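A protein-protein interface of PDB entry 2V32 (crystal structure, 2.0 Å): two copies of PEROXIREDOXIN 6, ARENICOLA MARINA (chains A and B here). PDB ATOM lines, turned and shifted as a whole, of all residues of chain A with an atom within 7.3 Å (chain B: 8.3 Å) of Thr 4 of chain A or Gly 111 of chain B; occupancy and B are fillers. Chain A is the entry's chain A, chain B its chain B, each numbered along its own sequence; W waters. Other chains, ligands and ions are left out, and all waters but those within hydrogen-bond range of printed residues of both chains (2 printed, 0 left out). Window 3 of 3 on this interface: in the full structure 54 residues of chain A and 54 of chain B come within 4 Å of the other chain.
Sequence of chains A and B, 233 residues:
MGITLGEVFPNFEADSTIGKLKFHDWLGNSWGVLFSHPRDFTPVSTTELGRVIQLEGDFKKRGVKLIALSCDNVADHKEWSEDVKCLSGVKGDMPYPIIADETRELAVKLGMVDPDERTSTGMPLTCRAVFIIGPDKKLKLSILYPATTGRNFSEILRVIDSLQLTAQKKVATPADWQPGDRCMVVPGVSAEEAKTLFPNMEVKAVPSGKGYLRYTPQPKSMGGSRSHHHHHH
Water W1 bridges the backbone carbonyl oxygen (O) of Val 113 of chain B and the backbone carbonyl oxygen (O) of Leu 5 of chain A.
Water W2 lies within hydrogen-bond range of O of Val 113 of chain B (2.8 Å), N of Leu 5 of chain A (2.9 Å) and O of Gly 111 of chain B (3.1 Å).
Positions printed for both chains: 2 and 3.
O of Ser 142 of chain A is in hydrogen-bond range of N of Leu 144 of chain B (2.7 Å).
Thr 4 of chain A touches one residue of chain B.
Printed residues of chain A within 4 Å of Pro 115 of chain B: Leu 5 and Gly 6.
Printed residues of chain A within 4 Å of Leu 144 of chain B: Leu 5 and Ser 142.
Of the printed residues of chain B, Leu 5 of chain A touches Pro 115 (3.7 Å), Leu 144 (3.8 Å) and Tyr 145 (3.97 Å).
Of the printed residues of chain B, Ser 142 of chain A touches Ile 143 and Leu 144.
Val 8 of chain A touches none of the printed residues of chain B.
The nearest residue of chain B that does not touch Thr 4 of chain A is Leu 144 of chain B (4.9 Å).
The nearest residue of chain A that does not touch Gly 111 of chain B is Leu 5 of chain A (5.1 Å).
The nearest printed residue of chain B that does not touch Gly 6 of chain A is Val 113 of chain B (6.4 Å).
Printed residues of chain A that touch a printed residue of chain B: Thr 4, Leu 5, Gly 6 and Ser 142.
N of Thr 4 of chain A lies within hydrogen-bond range of OE2 of Glu 7 of chain A (3.1 Å).
The backbone NH of Gly 6 of chain A sits at hydrogen-bond distance from the backbone carbonyl oxygen of Leu 139 of chain A.
Among the printed residues, merely in contact across the chains: Ser 142 of chain A with Ile 143 of chain B (3.5 Å), Gly 6 of chain A with Pro 115 of chain B (3.7 Å), Leu 5 of chain A with Pro 115 of chain B (3.7 Å), Thr 4 of chain A with Gly 111 of chain B (3.8 Å), Leu 5 of chain A with Leu 144 of chain B (3.8 Å) and Leu 5 of chain A with Tyr 145 of chain B (3.97 Å).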
ATOM      1  N   GLY A   2      -5.039   0.647   0.594  1.00  0.00           N
ATOM      2  CA  GLY A   2      -4.495   1.127   1.894  1.00  0.00           C
ATOM      3  C   GLY A   2      -4.887   2.553   2.186  1.00  0.00           C
ATOM      4  O   GLY A   2      -5.458   3.237   1.350  1.00  0.00           O
ATOM      5  N   ILE A   3      -4.578   3.019   3.380  1.00  0.00           N
ATOM      6  CA  ILE A   3      -4.976   4.349   3.810  1.00  0.00           C
ATOM      7  C   ILE A   3      -3.701   4.983   4.359  1.00  0.00           C
ATOM      8  O   ILE A   3      -2.963   4.318   5.108  1.00  0.00           O
ATOM      9  CB  ILE A   3      -6.081   4.243   4.831  1.00  0.00           C
ATOM     10  CG1 ILE A   3      -6.489   5.616   5.355  1.00  0.00           C
ATOM     11  CG2 ILE A   3      -5.687   3.265   5.939  1.00  0.00           C
ATOM     12  CD1 ILE A   3      -7.979   5.740   5.600  1.00  0.00           C
ATOM     13  N   THR A   4      -3.397   6.218   3.950  1.00  0.00           N
ATOM     14  CA  THR A   4      -2.183   6.870   4.404  1.00  0.00           C
ATOM     15  C   THR A   4      -2.612   7.904   5.406  1.00  0.00           C
ATOM     16  O   THR A   4      -3.804   8.247   5.510  1.00  0.00           O
ATOM     17  CB  THR A   4      -1.421   7.563   3.246  1.00  0.00           C
ATOM     18  OG1 THR A   4      -2.296   8.491   2.628  1.00  0.00           O
ATOM     19  CG2 THR A   4      -0.968   6.553   2.158  1.00  0.00           C
ATOM     20  N   LEU A   5      -1.655   8.398   6.174  1.00  0.00           N
ATOM     21  CA  LEU A   5      -1.940   9.392   7.187  1.00  0.00           C
ATOM     22  C   LEU A   5      -2.613  10.661   6.602  1.00  0.00           C
ATOM     23  O   LEU A   5      -2.319  11.057   5.464  1.00  0.00           O
ATOM     24  CB  LEU A   5      -0.684   9.714   7.972  1.00  0.00           C
ATOM     25  CG  LEU A   5       0.049   8.570   8.665  1.00  0.00           C
ATOM     26  CD1 LEU A   5       1.091   9.294   9.496  1.00  0.00           C
ATOM     27  CD2 LEU A   5      -0.931   7.783   9.613  1.00  0.00           C
ATOM     28  N   GLY A   6      -3.585  11.197   7.342  1.00  0.00           N
ATOM     29  CA  GLY A   6      -4.346  12.399   6.936  1.00  0.00           C
ATOM     30  C   GLY A   6      -5.466  12.192   5.911  1.00  0.00           C
ATOM     31  O   GLY A   6      -6.172  13.133   5.558  1.00  0.00           O
ATOM     32  N   GLU A   7      -5.618  10.957   5.422  1.00  0.00           N
ATOM     33  CA  GLU A   7      -6.750  10.616   4.570  1.00  0.00           C
ATOM     34  C   GLU A   7      -8.015  10.629   5.412  1.00  0.00           C
ATOM     35  O   GLU A   7      -7.947  10.246   6.598  1.00  0.00           O
ATOM     36  CB  GLU A   7      -6.577   9.223   4.030  1.00  0.00           C
ATOM     37  CG  GLU A   7      -5.760   9.178   2.787  1.00  0.00           C
ATOM     38  CD  GLU A   7      -6.037   7.905   1.954  1.00  0.00           C
ATOM     39  OE1 GLU A   7      -7.215   7.560   1.740  1.00  0.00           O
ATOM     40  OE2 GLU A   7      -5.054   7.275   1.504  1.00  0.00           O
ATOM     41  N   VAL A   8      -9.148  11.038   4.806  1.00  0.00           N
ATOM     42  CA  VAL A   8     -10.424  10.983   5.526  1.00  0.00           C
ATOM     43  C   VAL A   8     -10.704   9.467   5.599  1.00  0.00           C
ATOM     44  O   VAL A   8     -10.548   8.757   4.609  1.00  0.00           O
ATOM     45  CB  VAL A   8     -11.587  11.819   4.850  1.00  0.00           C
ATOM     46  CG1 VAL A   8     -12.922  11.613   5.607  1.00  0.00           C
ATOM     47  CG2 VAL A   8     -11.253  13.301   4.770  1.00  0.00           C
ATOM     48  N   PHE A   9     -10.969   8.942   6.787  1.00  0.00           N
ATOM     49  CA  PHE A   9     -11.228   7.494   6.912  1.00  0.00           C
ATOM     50  C   PHE A   9     -12.588   7.171   6.300  1.00  0.00           C
ATOM     51  O   PHE A   9     -13.518   7.928   6.477  1.00  0.00           O
ATOM     52  CB  PHE A   9     -11.235   7.113   8.409  1.00  0.00           C
ATOM     53  CG  PHE A   9     -10.814   5.693   8.682  1.00  0.00           C
ATOM     54  CD1 PHE A   9      -9.482   5.371   8.718  1.00  0.00           C
ATOM     55  CD2 PHE A   9     -11.770   4.690   8.927  1.00  0.00           C
ATOM     56  CE1 PHE A   9      -9.065   4.034   8.961  1.00  0.00           C
ATOM     57  CE2 PHE A   9     -11.390   3.386   9.181  1.00  0.00           C
ATOM     58  CZ  PHE A   9     -10.013   3.043   9.187  1.00  0.00           C
ATOM     59  N   LYS A 138     -10.088  12.067  10.076  1.00  0.00           N
ATOM     60  CA  LYS A 138      -8.850  11.802   9.356  1.00  0.00           C
ATOM     61  C   LYS A 138      -7.966  10.841  10.097  1.00  0.00           C
ATOM     62  O   LYS A 138      -7.891  10.880  11.329  1.00  0.00           O
ATOM     63  CB  LYS A 138      -8.121  13.091   9.112  1.00  0.00           C
ATOM     64  CG  LYS A 138      -8.891  14.010   8.220  1.00  0.00           C
ATOM     65  CD  LYS A 138      -8.112  15.256   7.963  1.00  0.00           C
ATOM     66  CE  LYS A 138      -8.929  16.245   7.075  1.00  0.00           C
ATOM     67  NZ  LYS A 138      -8.061  17.464   6.846  1.00  0.00           N
ATOM     68  N   LEU A 139      -7.305   9.967   9.355  1.00  0.00           N
ATOM     69  CA  LEU A 139      -6.341   8.993   9.940  1.00  0.00           C
ATOM     70  C   LEU A 139      -5.098   9.688  10.521  1.00  0.00           C
ATOM     71  O   LEU A 139      -4.379  10.383   9.794  1.00  0.00           O
ATOM     72  CB  LEU A 139      -5.948   7.899   8.905  1.00  0.00           C
ATOM     73  CG  LEU A 139      -4.804   7.003   9.384  1.00  0.00           C
ATOM     74  CD1 LEU A 139      -5.313   6.150  10.614  1.00  0.00           C
ATOM     75  CD2 LEU A 139      -4.384   6.062   8.263  1.00  0.00           C
ATOM     76  N   LYS A 140      -4.812   9.473  11.803  1.00  0.00           N
ATOM     77  CA  LYS A 140      -3.713  10.193  12.506  1.00  0.00           C
ATOM     78  C   LYS A 140      -2.458   9.345  12.748  1.00  0.00           C
ATOM     79  O   LYS A 140      -1.337   9.859  12.741  1.00  0.00           O
ATOM     80  CB  LYS A 140      -4.208  10.778  13.837  1.00  0.00           C
ATOM     81  CG  LYS A 140      -5.406  11.697  13.726  1.00  0.00           C
ATOM     82  CD  LYS A 140      -5.107  12.987  12.876  1.00  0.00           C
ATOM     83  CE  LYS A 140      -6.326  13.969  12.910  1.00  0.00           C
ATOM     84  NZ  LYS A 140      -6.320  14.942  11.750  1.00  0.00           N
ATOM     85  N   SER A 142      -1.142   4.849  12.411  1.00  0.00           N
ATOM     86  CA  SER A 142      -1.515   3.456  12.277  1.00  0.00           C
ATOM     87  C   SER A 142      -0.359   2.481  12.450  1.00  0.00           C
ATOM     88  O   SER A 142       0.829   2.841  12.241  1.00  0.00           O
ATOM     89  CB  SER A 142      -2.197   3.189  10.935  1.00  0.00           C
ATOM     90  OG  SER A 142      -1.324   3.429   9.875  1.00  0.00           O
ATOM     91  N   GLY B   2       0.977   2.221  -0.983  1.00  0.00           N
ATOM     92  CA  GLY B   2       1.326   1.652   0.364  1.00  0.00           C
ATOM     93  C   GLY B   2       1.928   0.315   0.141  1.00  0.00           C
ATOM     94  O   GLY B   2       1.918  -0.164  -0.976  1.00  0.00           O
ATOM     95  N   ILE B   3       2.521  -0.273   1.170  1.00  0.00           N
ATOM     96  CA  ILE B   3       3.033  -1.661   1.132  1.00  0.00           C
ATOM     97  C   ILE B   3       2.219  -2.375   2.233  1.00  0.00           C
ATOM     98  O   ILE B   3       1.812  -1.751   3.222  1.00  0.00           O
ATOM     99  CB  ILE B   3       4.586  -1.737   1.307  1.00  0.00           C
ATOM    100  CG1 ILE B   3       5.082  -3.187   1.381  1.00  0.00           C
ATOM    101  CG2 ILE B   3       5.054  -0.952   2.497  1.00  0.00           C
ATOM    102  CD1 ILE B   3       6.571  -3.363   1.105  1.00  0.00           C
ATOM    103  N   ARG B 104      11.367  11.848  -3.619  1.00  0.00           N
ATOM    104  CA  ARG B 104      10.079  11.493  -2.994  1.00  0.00           C
ATOM    105  C   ARG B 104       9.520  10.201  -3.553  1.00  0.00           C
ATOM    106  O   ARG B 104       8.338   9.859  -3.336  1.00  0.00           O
ATOM    107  CB  ARG B 104       9.040  12.622  -3.155  1.00  0.00           C
ATOM    108  CG  ARG B 104       9.042  13.632  -2.041  1.00  0.00           C
ATOM    109  CD  ARG B 104      10.259  14.514  -2.080  1.00  0.00           C
ATOM    110  NE  ARG B 104      10.248  15.575  -1.058  1.00  0.00           N
ATOM    111  CZ  ARG B 104      11.230  16.455  -0.868  1.00  0.00           C
ATOM    112  NH1 ARG B 104      12.361  16.392  -1.605  1.00  0.00           N
ATOM    113  NH2 ARG B 104      11.114  17.378   0.101  1.00  0.00           N
ATOM    114  N   GLU B 105      10.380   9.431  -4.223  1.00  0.00           N
ATOM    115  CA  GLU B 105       9.868   8.252  -4.858  1.00  0.00           C
ATOM    116  C   GLU B 105       9.507   7.145  -3.879  1.00  0.00           C
ATOM    117  O   GLU B 105       8.506   6.476  -4.083  1.00  0.00           O
ATOM    118  CB  GLU B 105      10.744   7.792  -6.037  1.00  0.00           C
ATOM    119  CG  GLU B 105      10.478   8.717  -7.309  1.00  0.00           C
ATOM    120  CD  GLU B 105       8.954   9.060  -7.606  1.00  0.00           C
ATOM    121  OE1 GLU B 105       8.207   8.166  -8.117  1.00  0.00           O
ATOM    122  OE2 GLU B 105       8.527  10.235  -7.330  1.00  0.00           O
ATOM    123  N   LEU B 106      10.293   7.040  -2.805  1.00  0.00           N
ATOM    124  CA  LEU B 106      10.117   6.072  -1.731  1.00  0.00           C
ATOM    125  C   LEU B 106       9.075   6.559  -0.789  1.00  0.00           C
ATOM    126  O   LEU B 106       8.297   5.799  -0.313  1.00  0.00           O
ATOM    127  CB  LEU B 106      11.429   5.892  -0.981  1.00  0.00           C
ATOM    128  CG  LEU B 106      12.530   5.174  -1.784  1.00  0.00           C
ATOM    129  CD1 LEU B 106      13.919   5.321  -1.148  1.00  0.00           C
ATOM    130  CD2 LEU B 106      12.121   3.705  -2.128  1.00  0.00           C
ATOM    131  N   ALA B 107       9.020   7.849  -0.555  1.00  0.00           N
ATOM    132  CA  ALA B 107       7.968   8.449   0.307  1.00  0.00           C
ATOM    133  C   ALA B 107       6.608   8.122  -0.250  1.00  0.00           C
ATOM    134  O   ALA B 107       5.695   7.750   0.491  1.00  0.00           O
ATOM    135  CB  ALA B 107       8.158   9.958   0.398  1.00  0.00           C
ATOM    136  N   VAL B 108       6.463   8.231  -1.583  1.00  0.00           N
ATOM    137  CA  VAL B 108       5.215   7.834  -2.244  1.00  0.00           C
ATOM    138  C   VAL B 108       5.011   6.301  -2.341  1.00  0.00           C
ATOM    139  O   VAL B 108       3.921   5.779  -2.038  1.00  0.00           O
ATOM    140  CB  VAL B 108       5.015   8.544  -3.621  1.00  0.00           C
ATOM    141  CG1 VAL B 108       3.600   8.279  -4.095  1.00  0.00           C
ATOM    142  CG2 VAL B 108       5.170  10.040  -3.463  1.00  0.00           C
ATOM    143  N   LYS B 109       6.045   5.573  -2.786  1.00  0.00           N
ATOM    144  CA  LYS B 109       5.927   4.119  -2.893  1.00  0.00           C
ATOM    145  C   LYS B 109       5.561   3.477  -1.561  1.00  0.00           C
ATOM    146  O   LYS B 109       4.754   2.553  -1.533  1.00  0.00           O
ATOM    147  CB  LYS B 109       7.201   3.475  -3.398  1.00  0.00           C
ATOM    148  CG  LYS B 109       6.963   2.143  -4.059  1.00  0.00           C
ATOM    149  CD  LYS B 109       8.309   1.461  -4.405  1.00  0.00           C
ATOM    150  CE  LYS B 109       8.992   1.975  -5.682  1.00  0.00           C
ATOM    151  NZ  LYS B 109      10.500   1.734  -5.617  1.00  0.00           N
ATOM    152  N   LEU B 110       6.166   3.950  -0.462  1.00  0.00           N
ATOM    153  CA  LEU B 110       5.954   3.300   0.826  1.00  0.00           C
ATOM    154  C   LEU B 110       4.701   3.720   1.579  1.00  0.00           C
ATOM    155  O   LEU B 110       4.419   3.136   2.633  1.00  0.00           O
ATOM    156  CB  LEU B 110       7.191   3.372   1.692  1.00  0.00           C
ATOM    157  CG  LEU B 110       8.436   2.710   1.051  1.00  0.00           C
ATOM    158  CD1 LEU B 110       9.609   2.790   1.945  1.00  0.00           C
ATOM    159  CD2 LEU B 110       8.196   1.271   0.758  1.00  0.00           C
ATOM    160  N   GLY B 111       3.943   4.688   1.052  1.00  0.00           N
ATOM    161  CA  GLY B 111       2.732   5.199   1.739  1.00  0.00           C
ATOM    162  C   GLY B 111       3.067   5.957   3.026  1.00  0.00           C
ATOM    163  O   GLY B 111       2.276   5.960   4.005  1.00  0.00           O
ATOM    164  N   MET B 112       4.211   6.646   3.004  1.00  0.00           N
ATOM    165  CA  MET B 112       4.783   7.259   4.207  1.00  0.00           C
ATOM    166  C   MET B 112       4.924   8.781   4.149  1.00  0.00           C
ATOM    167  O   MET B 112       5.716   9.333   4.900  1.00  0.00           O
ATOM    168  CB  MET B 112       6.142   6.598   4.587  1.00  0.00           C
ATOM    169  CG  MET B 112       7.356   7.100   3.791  1.00  0.00           C
ATOM    170  SD  MET B 112       8.833   6.161   4.256  1.00  0.00           S
ATOM    171  CE  MET B 112       9.952   6.500   2.905  1.00  0.00           C
ATOM    172  N   VAL B 113       4.145   9.447   3.307  1.00  0.00           N
ATOM    173  CA  VAL B 113       4.136  10.907   3.230  1.00  0.00           C
ATOM    174  C   VAL B 113       3.441  11.448   4.512  1.00  0.00           C
ATOM    175  O   VAL B 113       2.369  10.936   4.890  1.00  0.00           O
ATOM    176  CB  VAL B 113       3.412  11.414   1.914  1.00  0.00           C
ATOM    177  CG1 VAL B 113       3.154  12.946   1.941  1.00  0.00           C
ATOM    178  CG2 VAL B 113       4.195  11.024   0.660  1.00  0.00           C
ATOM    179  N   ASP B 114       4.057  12.457   5.141  1.00  0.00           N
ATOM    180  CA  ASP B 114       3.477  13.108   6.323  1.00  0.00           C
ATOM    181  C   ASP B 114       2.240  13.919   5.971  1.00  0.00           C
ATOM    182  O   ASP B 114       2.236  14.631   4.956  1.00  0.00           O
ATOM    183  CB  ASP B 114       4.479  14.036   7.039  1.00  0.00           C
ATOM    184  CG  ASP B 114       4.004  14.417   8.417  1.00  0.00           C
ATOM    185  OD1 ASP B 114       4.274  13.650   9.370  1.00  0.00           O
ATOM    186  OD2 ASP B 114       3.381  15.490   8.584  1.00  0.00           O
ATOM    187  N   PRO B 115       1.195  13.857   6.823  1.00  0.00           N
ATOM    188  CA  PRO B 115      -0.007  14.618   6.491  1.00  0.00           C
ATOM    189  C   PRO B 115       0.051  16.139   6.688  1.00  0.00           C
ATOM    190  O   PRO B 115      -0.794  16.818   6.118  1.00  0.00           O
ATOM    191  CB  PRO B 115      -1.067  14.014   7.414  1.00  0.00           C
ATOM    192  CG  PRO B 115      -0.336  13.352   8.479  1.00  0.00           C
ATOM    193  CD  PRO B 115       1.037  13.069   8.057  1.00  0.00           C
ATOM    194  N   THR B 126       8.397  12.706   4.440  1.00  0.00           N
ATOM    195  CA  THR B 126       8.042  11.423   5.124  1.00  0.00           C
ATOM    196  C   THR B 126       7.521  11.709   6.540  1.00  0.00           C
ATOM    197  O   THR B 126       7.812  12.747   7.146  1.00  0.00           O
ATOM    198  CB  THR B 126       9.253  10.429   5.227  1.00  0.00           C
ATOM    199  OG1 THR B 126      10.309  11.033   5.969  1.00  0.00           O
ATOM    200  CG2 THR B 126       9.854  10.114   3.793  1.00  0.00           C
ATOM    201  N   CYS B 127       6.725  10.781   7.044  1.00  0.00           N
ATOM    202  CA  CYS B 127       6.297  10.817   8.425  1.00  0.00           C
ATOM    203  C   CYS B 127       7.394  10.056   9.218  1.00  0.00           C
ATOM    204  O   CYS B 127       8.513   9.925   8.740  1.00  0.00           O
ATOM    205  CB  CYS B 127       4.929  10.137   8.543  1.00  0.00           C
ATOM    206  SG  CYS B 127       4.768   8.393   7.954  1.00  0.00           S
ATOM    207  N   ALA B 129       7.968   6.645   9.978  1.00  0.00           N
ATOM    208  CA  ALA B 129       7.537   5.324   9.606  1.00  0.00           C
ATOM    209  C   ALA B 129       8.597   4.312  10.030  1.00  0.00           C
ATOM    210  O   ALA B 129       9.792   4.675  10.207  1.00  0.00           O
ATOM    211  CB  ALA B 129       7.227   5.247   8.099  1.00  0.00           C
ATOM    212  N   PHE B 131       9.550   0.146   9.077  1.00  0.00           N
ATOM    213  CA  PHE B 131       9.306  -1.084   8.343  1.00  0.00           C
ATOM    214  C   PHE B 131      10.280  -2.165   8.810  1.00  0.00           C
ATOM    215  O   PHE B 131      11.492  -2.007   8.672  1.00  0.00           O
ATOM    216  CB  PHE B 131       9.422  -0.858   6.801  1.00  0.00           C
ATOM    217  CG  PHE B 131       8.456   0.172   6.256  1.00  0.00           C
ATOM    218  CD1 PHE B 131       7.125  -0.140   6.032  1.00  0.00           C
ATOM    219  CD2 PHE B 131       8.869   1.482   6.034  1.00  0.00           C
ATOM    220  CE1 PHE B 131       6.232   0.833   5.602  1.00  0.00           C
ATOM    221  CE2 PHE B 131       7.987   2.458   5.584  1.00  0.00           C
ATOM    222  CZ  PHE B 131       6.675   2.148   5.379  1.00  0.00           C
ATOM    223  N   ILE B 143       4.722   0.532  11.139  1.00  0.00           N
ATOM    224  CA  ILE B 143       4.036   1.611  11.905  1.00  0.00           C
ATOM    225  C   ILE B 143       4.162   2.921  11.154  1.00  0.00           C
ATOM    226  O   ILE B 143       5.212   3.197  10.566  1.00  0.00           O
ATOM    227  CB  ILE B 143       4.584   1.813  13.340  1.00  0.00           C
ATOM    228  CG1 ILE B 143       5.978   2.467  13.320  1.00  0.00           C
ATOM    229  CG2 ILE B 143       4.510   0.513  14.187  1.00  0.00           C
ATOM    230  CD1 ILE B 143       6.540   2.842  14.710  1.00  0.00           C
ATOM    231  N   LEU B 144       3.085   3.708  11.125  1.00  0.00           N
ATOM    232  CA  LEU B 144       3.093   5.047  10.536  1.00  0.00           C
ATOM    233  C   LEU B 144       2.661   6.042  11.600  1.00  0.00           C
ATOM    234  O   LEU B 144       1.472   6.098  12.009  1.00  0.00           O
ATOM    235  CB  LEU B 144       2.172   5.125   9.313  1.00  0.00           C
ATOM    236  CG  LEU B 144       2.403   4.293   8.051  1.00  0.00           C
ATOM    237  CD1 LEU B 144       1.251   4.585   7.133  1.00  0.00           C
ATOM    238  CD2 LEU B 144       3.701   4.647   7.347  1.00  0.00           C
ATOM    239  N   TYR B 145       3.647   6.774  12.102  1.00  0.00           N
ATOM    240  CA  TYR B 145       3.460   7.775  13.139  1.00  0.00           C
ATOM    241  C   TYR B 145       3.683   9.122  12.495  1.00  0.00           C
ATOM    242  O   TYR B 145       4.655   9.286  11.722  1.00  0.00           O
ATOM    243  CB  TYR B 145       4.496   7.644  14.259  1.00  0.00           C
ATOM    244  CG  TYR B 145       4.256   6.626  15.368  1.00  0.00           C
ATOM    245  CD1 TYR B 145       3.379   5.506  15.185  1.00  0.00           C
ATOM    246  CD2 TYR B 145       4.908   6.775  16.615  1.00  0.00           C
ATOM    247  CE1 TYR B 145       3.215   4.573  16.174  1.00  0.00           C
ATOM    248  CE2 TYR B 145       4.742   5.798  17.638  1.00  0.00           C
ATOM    249  CZ  TYR B 145       3.897   4.698  17.379  1.00  0.00           C
ATOM    250  OH  TYR B 145       3.690   3.715  18.371  1.00  0.00           O
HETATM  251  O   HOH W   1       0.069  11.635   3.943  1.00  0.00           O
HETATM  252  O   HOH W   2       1.106   8.473   5.348  1.00  0.00           O
